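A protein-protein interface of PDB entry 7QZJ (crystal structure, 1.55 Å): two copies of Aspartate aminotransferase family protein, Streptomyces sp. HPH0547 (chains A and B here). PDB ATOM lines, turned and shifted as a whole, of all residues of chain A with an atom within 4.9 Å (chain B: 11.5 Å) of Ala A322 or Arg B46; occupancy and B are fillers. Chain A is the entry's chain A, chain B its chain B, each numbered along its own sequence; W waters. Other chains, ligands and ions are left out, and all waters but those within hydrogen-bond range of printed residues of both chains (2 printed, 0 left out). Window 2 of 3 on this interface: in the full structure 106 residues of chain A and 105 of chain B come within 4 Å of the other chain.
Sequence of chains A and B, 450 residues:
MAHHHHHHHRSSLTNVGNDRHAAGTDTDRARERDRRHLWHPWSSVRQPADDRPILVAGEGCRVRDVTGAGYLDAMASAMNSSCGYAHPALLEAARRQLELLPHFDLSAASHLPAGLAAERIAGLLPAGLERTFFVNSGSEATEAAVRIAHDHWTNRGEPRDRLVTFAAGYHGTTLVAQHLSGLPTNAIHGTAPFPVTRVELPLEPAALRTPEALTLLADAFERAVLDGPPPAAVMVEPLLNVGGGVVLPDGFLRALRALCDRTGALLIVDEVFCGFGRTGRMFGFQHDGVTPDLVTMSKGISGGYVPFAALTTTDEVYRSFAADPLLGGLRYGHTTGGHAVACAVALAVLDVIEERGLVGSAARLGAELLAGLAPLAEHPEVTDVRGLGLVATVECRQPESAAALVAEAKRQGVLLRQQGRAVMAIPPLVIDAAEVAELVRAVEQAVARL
No position is printed for both chains. Of the 9 pairs that touch across the chains among the printed residues, none has its exchanged pair printed and touching as well.
Printed residues of chain B within 4 Å of Arg A319: Val B45. Of the printed residues of chain B, Phe A321 touches Trp B39 (3.8 Å) and Val B45 (3.8 Å). Of chain B, only Val B45 and Arg B46 come within 4 Å of Ala A322. Gly A328 touches two residues of chain B. Arg B35 touches none of the printed residues of chain A. Printed residues of chain A within 4 Å of Trp B39: Tyr A318 (3.6 Å) and Phe A321 (3.8 Å). Printed residues of chain A within 4 Å of Ser B44: Gly A328. Printed residues of chain A within 4 Å of Val B45: Tyr A318, Arg A319, Phe A321, Ala A322 and Gly A328. Printed residues of chain A within 4 Å of Arg B46: Ala A322. The nearest residue of chain B that does not touch Ala A322 is Ser B44 (6.7 Å). The nearest printed residue of chain A that does not touch Val B45 is Ser A320 (5.9 Å).
CE2 of Trp B39 touches CD1 of Tyr A318, at 3.6 Å. Tyr A318 touches Val B45 (O to CG2, 3.6 Å). Arg A319 touches Val B45 (NH2 to CG1, 3.7 Å). Trp B39 touches Phe A321. Phe A321 touches Val B45. Ala A322 touches Val B45 (N to CG2, 3.9 Å). Arg B46 touches Ala A322. CA of Ser B44 touches O of Gly A328 (3.5 Å).
Water W2 lies within hydrogen-bond range of O of Gly A328 (2.8 Å), N of Arg B46 (3.0 Å) and N of Val B45 (3.5 Å). Water W1 bridges the side-chain hydroxyl (OH) of Tyr A318 (2.9 Å) and the backbone NH (N) of His B40 (3.1 Å).
Printed residues of chain A that touch a printed residue of chain B: Tyr A318, Arg A319, Phe A321, Ala A322 and Gly A328. Hydrophobic or aromatic side chains of chain A within 4 Å of the printed part of chain B: Tyr A318, Phe A321 and Ala A322. Hydrophobic or aromatic side chains of chain B that line the printed part of chain A: Trp B39 and Val B45. Among the printed residues, 9 pairs touch across the chains. Among the printed residues, no Asp or Glu carboxylate lies within 4 Å of a Lys or Arg side-chain nitrogen of the other chain.
O of Gly A328 is in hydrogen-bond range of N of Val B45.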
ATOM      1  N   TYR A 318      24.041   7.991   5.383  1.00  0.00           N
ATOM      2  CA  TYR A 318      24.295   8.219   6.800  1.00  0.00           C
ATOM      3  C   TYR A 318      23.461   9.356   7.372  1.00  0.00           C
ATOM      4  O   TYR A 318      22.687   9.153   8.305  1.00  0.00           O
ATOM      5  CB  TYR A 318      25.785   8.495   7.012  1.00  0.00           C
ATOM      6  CG  TYR A 318      26.177   8.816   8.423  1.00  0.00           C
ATOM      7  CD1 TYR A 318      26.133   7.837   9.417  1.00  0.00           C
ATOM      8  CD2 TYR A 318      26.570  10.100   8.790  1.00  0.00           C
ATOM      9  CE1 TYR A 318      26.487   8.126  10.712  1.00  0.00           C
ATOM     10  CE2 TYR A 318      26.927  10.399  10.090  1.00  0.00           C
ATOM     11  CZ  TYR A 318      26.891   9.400  11.052  1.00  0.00           C
ATOM     12  OH  TYR A 318      27.249   9.685  12.338  1.00  0.00           O
ATOM     13  N   ARG A 319      23.584  10.543   6.776  1.00  0.00           N
ATOM     14  CA  ARG A 319      22.958  11.741   7.334  1.00  0.00           C
ATOM     15  C   ARG A 319      21.438  11.692   7.290  1.00  0.00           C
ATOM     16  O   ARG A 319      20.812  12.349   8.102  1.00  0.00           O
ATOM     17  CB  ARG A 319      23.427  13.001   6.601  1.00  0.00           C
ATOM     18  CG  ARG A 319      24.898  13.316   6.796  1.00  0.00           C
ATOM     19  CD  ARG A 319      25.163  14.156   8.034  1.00  0.00           C
ATOM     20  NE  ARG A 319      26.590  14.124   8.379  1.00  0.00           N
ATOM     21  CZ  ARG A 319      27.098  14.208   9.610  1.00  0.00           C
ATOM     22  NH1 ARG A 319      28.419  14.155   9.776  1.00  0.00           N
ATOM     23  NH2 ARG A 319      26.314  14.331  10.682  1.00  0.00           N
ATOM     24  N   SER A 320      20.882  10.921   6.352  1.00  0.00           N
ATOM     25  CA  SER A 320      19.426  10.750   6.209  1.00  0.00           C
ATOM     26  C   SER A 320      18.797  10.211   7.481  1.00  0.00           C
ATOM     27  O   SER A 320      17.632  10.468   7.751  1.00  0.00           O
ATOM     28  CB  SER A 320      19.059   9.831   5.027  1.00  0.00           C
ATOM     29  OG  SER A 320      19.212   8.400   5.276  1.00  0.00           O
ATOM     30  N   PHE A 321      19.580   9.477   8.269  1.00  0.00           N
ATOM     31  CA  PHE A 321      19.102   8.928   9.532  1.00  0.00           C
ATOM     32  C   PHE A 321      18.791   9.954  10.605  1.00  0.00           C
ATOM     33  O   PHE A 321      18.093   9.630  11.543  1.00  0.00           O
ATOM     34  CB  PHE A 321      20.030   7.783  10.028  1.00  0.00           C
ATOM     35  CG  PHE A 321      19.818   6.522   9.250  1.00  0.00           C
ATOM     36  CD1 PHE A 321      20.460   6.326   8.031  1.00  0.00           C
ATOM     37  CD2 PHE A 321      18.887   5.585   9.657  1.00  0.00           C
ATOM     38  CE1 PHE A 321      20.182   5.231   7.238  1.00  0.00           C
ATOM     39  CE2 PHE A 321      18.621   4.476   8.865  1.00  0.00           C
ATOM     40  CZ  PHE A 321      19.262   4.297   7.655  1.00  0.00           C
ATOM     41  N   ALA A 322      19.239  11.204  10.454  1.00  0.00           N
ATOM     42  CA  ALA A 322      18.767  12.261  11.330  1.00  0.00           C
ATOM     43  C   ALA A 322      17.228  12.433  11.269  1.00  0.00           C
ATOM     44  O   ALA A 322      16.647  12.944  12.221  1.00  0.00           O
ATOM     45  CB  ALA A 322      19.477  13.574  11.023  1.00  0.00           C
ATOM     46  N   ALA A 323      16.587  11.984  10.188  1.00  0.00           N
ATOM     47  CA  ALA A 323      15.117  12.004  10.042  1.00  0.00           C
ATOM     48  C   ALA A 323      14.380  10.829  10.707  1.00  0.00           C
ATOM     49  O   ALA A 323      13.149  10.836  10.757  1.00  0.00           O
ATOM     50  CB  ALA A 323      14.739  12.062   8.571  1.00  0.00           C
ATOM     51  N   ASP A 324      15.110   9.808  11.183  1.00  0.00           N
ATOM     52  CA  ASP A 324      14.468   8.699  11.910  1.00  0.00           C
ATOM     53  C   ASP A 324      13.730   9.263  13.120  1.00  0.00           C
ATOM     54  O   ASP A 324      14.343   9.881  13.967  1.00  0.00           O
ATOM     55  CB  ASP A 324      15.518   7.661  12.350  1.00  0.00           C
ATOM     56  CG  ASP A 324      14.895   6.469  13.060  1.00  0.00           C
ATOM     57  OD1 ASP A 324      14.589   6.585  14.252  1.00  0.00           O
ATOM     58  OD2 ASP A 324      14.749   5.407  12.413  1.00  0.00           O
ATOM     59  N   GLY A 328      16.577   9.246  15.646  1.00  0.00           N
ATOM     60  CA  GLY A 328      17.458  10.212  14.973  1.00  0.00           C
ATOM     61  C   GLY A 328      18.749   9.567  14.493  1.00  0.00           C
ATOM     62  O   GLY A 328      19.734  10.234  14.203  1.00  0.00           O
ATOM     63  N   ARG B  35      34.657  10.728  13.974  1.00  0.00           N
ATOM     64  CA  ARG B  35      33.586  11.610  13.493  1.00  0.00           C
ATOM     65  C   ARG B  35      33.345  11.450  12.001  1.00  0.00           C
ATOM     66  O   ARG B  35      32.199  11.472  11.539  1.00  0.00           O
ATOM     67  CB  ARG B  35      33.935  13.069  13.800  1.00  0.00           C
ATOM     68  CG  ARG B  35      32.787  14.046  13.601  1.00  0.00           C
ATOM     69  CD  ARG B  35      33.166  15.445  14.082  1.00  0.00           C
ATOM     70  NE  ARG B  35      34.028  16.154  13.133  1.00  0.00           N
ATOM     71  CZ  ARG B  35      33.609  16.884  12.094  1.00  0.00           C
ATOM     72  NH1 ARG B  35      32.314  17.038  11.823  1.00  0.00           N
ATOM     73  NH2 ARG B  35      34.507  17.480  11.312  1.00  0.00           N
ATOM     74  N   LEU B  38      33.394   6.527  11.354  1.00  0.00           N
ATOM     75  CA  LEU B  38      32.790   5.457  12.173  1.00  0.00           C
ATOM     76  C   LEU B  38      31.289   5.688  12.340  1.00  0.00           C
ATOM     77  O   LEU B  38      30.845   6.785  12.712  1.00  0.00           O
ATOM     78  CB  LEU B  38      33.475   5.358  13.537  1.00  0.00           C
ATOM     79  CG  LEU B  38      33.034   4.205  14.463  1.00  0.00           C
ATOM     80  CD1 LEU B  38      33.175   2.830  13.827  1.00  0.00           C
ATOM     81  CD2 LEU B  38      33.821   4.261  15.761  1.00  0.00           C
ATOM     82  N   TRP B  39      30.507   4.642  12.068  1.00  0.00           N
ATOM     83  CA  TRP B  39      29.070   4.648  12.304  1.00  0.00           C
ATOM     84  C   TRP B  39      28.810   3.886  13.609  1.00  0.00           C
ATOM     85  O   TRP B  39      29.008   2.660  13.665  1.00  0.00           O
ATOM     86  CB  TRP B  39      28.336   3.995  11.138  1.00  0.00           C
ATOM     87  CG  TRP B  39      26.871   4.340  11.049  1.00  0.00           C
ATOM     88  CD1 TRP B  39      26.057   4.801  12.055  1.00  0.00           C
ATOM     89  CD2 TRP B  39      26.047   4.230   9.893  1.00  0.00           C
ATOM     90  NE1 TRP B  39      24.776   4.988  11.574  1.00  0.00           N
ATOM     91  CE2 TRP B  39      24.746   4.637  10.256  1.00  0.00           C
ATOM     92  CE3 TRP B  39      26.278   3.811   8.582  1.00  0.00           C
ATOM     93  CZ2 TRP B  39      23.698   4.706   9.327  1.00  0.00           C
ATOM     94  CZ3 TRP B  39      25.234   3.849   7.677  1.00  0.00           C
ATOM     95  CH2 TRP B  39      23.957   4.286   8.057  1.00  0.00           C
ATOM     96  N   HIS B  40      28.417   4.606  14.659  1.00  0.00           N
ATOM     97  CA  HIS B  40      28.146   3.989  15.966  1.00  0.00           C
ATOM     98  C   HIS B  40      26.781   3.297  15.997  1.00  0.00           C
ATOM     99  O   HIS B  40      25.825   3.768  15.372  1.00  0.00           O
ATOM    100  CB  HIS B  40      28.223   5.054  17.058  1.00  0.00           C
ATOM    101  CG  HIS B  40      29.601   5.616  17.242  1.00  0.00           C
ATOM    102  ND1 HIS B  40      30.426   5.246  18.282  1.00  0.00           N
ATOM    103  CD2 HIS B  40      30.293   6.528  16.518  1.00  0.00           C
ATOM    104  CE1 HIS B  40      31.574   5.895  18.180  1.00  0.00           C
ATOM    105  NE2 HIS B  40      31.521   6.669  17.114  1.00  0.00           N
ATOM    106  N   PRO B  41      26.678   2.200  16.762  1.00  0.00           N
ATOM    107  CA  PRO B  41      25.419   1.474  16.927  1.00  0.00           C
ATOM    108  C   PRO B  41      24.472   2.255  17.831  1.00  0.00           C
ATOM    109  O   PRO B  41      24.923   2.993  18.744  1.00  0.00           O
ATOM    110  CB  PRO B  41      25.866   0.168  17.592  1.00  0.00           C
ATOM    111  CG  PRO B  41      27.031   0.584  18.422  1.00  0.00           C
ATOM    112  CD  PRO B  41      27.755   1.606  17.587  1.00  0.00           C
ATOM    113  N   TRP B  42      23.181   2.130  17.560  1.00  0.00           N
ATOM    114  CA  TRP B  42      22.130   2.618  18.476  1.00  0.00           C
ATOM    115  C   TRP B  42      22.357   4.063  18.936  1.00  0.00           C
ATOM    116  O   TRP B  42      22.252   4.377  20.129  1.00  0.00           O
ATOM    117  CB  TRP B  42      21.988   1.650  19.663  1.00  0.00           C
ATOM    118  CG  TRP B  42      21.358   0.343  19.244  1.00  0.00           C
ATOM    119  CD1 TRP B  42      21.962  -0.878  19.196  1.00  0.00           C
ATOM    120  CD2 TRP B  42      20.005   0.133  18.814  1.00  0.00           C
ATOM    121  NE1 TRP B  42      21.082  -1.832  18.776  1.00  0.00           N
ATOM    122  CE2 TRP B  42      19.872  -1.243  18.523  1.00  0.00           C
ATOM    123  CE3 TRP B  42      18.884   0.961  18.685  1.00  0.00           C
ATOM    124  CZ2 TRP B  42      18.673  -1.804  18.098  1.00  0.00           C
ATOM    125  CZ3 TRP B  42      17.703   0.405  18.240  1.00  0.00           C
ATOM    126  CH2 TRP B  42      17.603  -0.966  17.949  1.00  0.00           C
ATOM    127  N   SER B  43      22.692   4.922  17.970  1.00  0.00           N
ATOM    128  CA  SER B  43      23.097   6.300  18.237  1.00  0.00           C
ATOM    129  C   SER B  43      22.432   7.288  17.308  1.00  0.00           C
ATOM    130  O   SER B  43      22.135   6.975  16.177  1.00  0.00           O
ATOM    131  CB  SER B  43      24.603   6.433  18.065  1.00  0.00           C
ATOM    132  OG  SER B  43      25.264   5.739  19.109  1.00  0.00           O
ATOM    133  N   SER B  44      22.261   8.511  17.798  1.00  0.00           N
ATOM    134  CA  SER B  44      21.779   9.604  16.967  1.00  0.00           C
ATOM    135  C   SER B  44      22.897  10.097  16.073  1.00  0.00           C
ATOM    136  O   SER B  44      24.062  10.145  16.482  1.00  0.00           O
ATOM    137  CB  SER B  44      21.283  10.767  17.829  1.00  0.00           C
ATOM    138  OG  SER B  44      20.060  10.399  18.417  1.00  0.00           O
ATOM    139  N   VAL B  45      22.526  10.442  14.847  1.00  0.00           N
ATOM    140  CA  VAL B  45      23.434  11.071  13.887  1.00  0.00           C
ATOM    141  C   VAL B  45      23.939  12.428  14.403  1.00  0.00           C
ATOM    142  O   VAL B  45      25.111  12.749  14.222  1.00  0.00           O
ATOM    143  CB  VAL B  45      22.747  11.202  12.505  1.00  0.00           C
ATOM    144  CG1 VAL B  45      23.485  12.161  11.570  1.00  0.00           C
ATOM    145  CG2 VAL B  45      22.652   9.830  11.875  1.00  0.00           C
ATOM    146  N   ARG B  46      23.079  13.193  15.072  1.00  0.00           N
ATOM    147  CA  ARG B  46      23.447  14.546  15.527  1.00  0.00           C
ATOM    148  C   ARG B  46      23.924  14.604  16.986  1.00  0.00           C
ATOM    149  O   ARG B  46      23.304  14.034  17.881  1.00  0.00           O
ATOM    150  CB  ARG B  46      22.277  15.493  15.275  1.00  0.00           C
ATOM    151  CG  ARG B  46      22.088  15.767  13.790  1.00  0.00           C
ATOM    152  CD  ARG B  46      20.785  16.478  13.485  1.00  0.00           C
ATOM    153  NE  ARG B  46      20.602  16.621  12.041  1.00  0.00           N
ATOM    154  CZ  ARG B  46      19.465  16.964  11.442  1.00  0.00           C
ATOM    155  NH1 ARG B  46      19.430  17.058  10.114  1.00  0.00           N
ATOM    156  NH2 ARG B  46      18.355  17.193  12.143  1.00  0.00           N
ATOM    157  N   ASP B  51      31.072  15.057  23.995  1.00  0.00           N
ATOM    158  CA  ASP B  51      31.354  13.947  23.084  1.00  0.00           C
ATOM    159  C   ASP B  51      31.847  12.670  23.816  1.00  0.00           C
ATOM    160  O   ASP B  51      32.105  12.683  25.030  1.00  0.00           O
ATOM    161  CB  ASP B  51      32.332  14.395  21.982  1.00  0.00           C
ATOM    162  CG  ASP B  51      33.571  15.075  22.530  1.00  0.00           C
ATOM    163  OD1 ASP B  51      34.366  15.601  21.717  1.00  0.00           O
ATOM    164  OD2 ASP B  51      33.756  15.096  23.765  1.00  0.00           O
ATOM    165  N   ARG B  52      31.964  11.577  23.062  1.00  0.00           N
ATOM    166  CA  ARG B  52      32.144  10.237  23.629  1.00  0.00           C
ATOM    167  C   ARG B  52      33.525  10.015  24.238  1.00  0.00           C
ATOM    168  O   ARG B  52      34.526  10.391  23.622  1.00  0.00           O
ATOM    169  CB  ARG B  52      31.959   9.180  22.537  1.00  0.00           C
ATOM    170  CG  ARG B  52      30.560   9.110  21.950  1.00  0.00           C
ATOM    171  CD  ARG B  52      30.362   7.819  21.173  1.00  0.00           C
ATOM    172  NE  ARG B  52      29.013   7.701  20.620  1.00  0.00           N
ATOM    173  CZ  ARG B  52      28.579   8.297  19.508  1.00  0.00           C
ATOM    174  NH1 ARG B  52      29.370   9.096  18.779  1.00  0.00           N
ATOM    175  NH2 ARG B  52      27.325   8.096  19.118  1.00  0.00           N
HETATM  176  O   HOH W   1      27.795   7.587  14.327  1.00  0.00           O
HETATM  177  O   HOH W   2      20.063  12.897  14.901  1.00  0.00           O
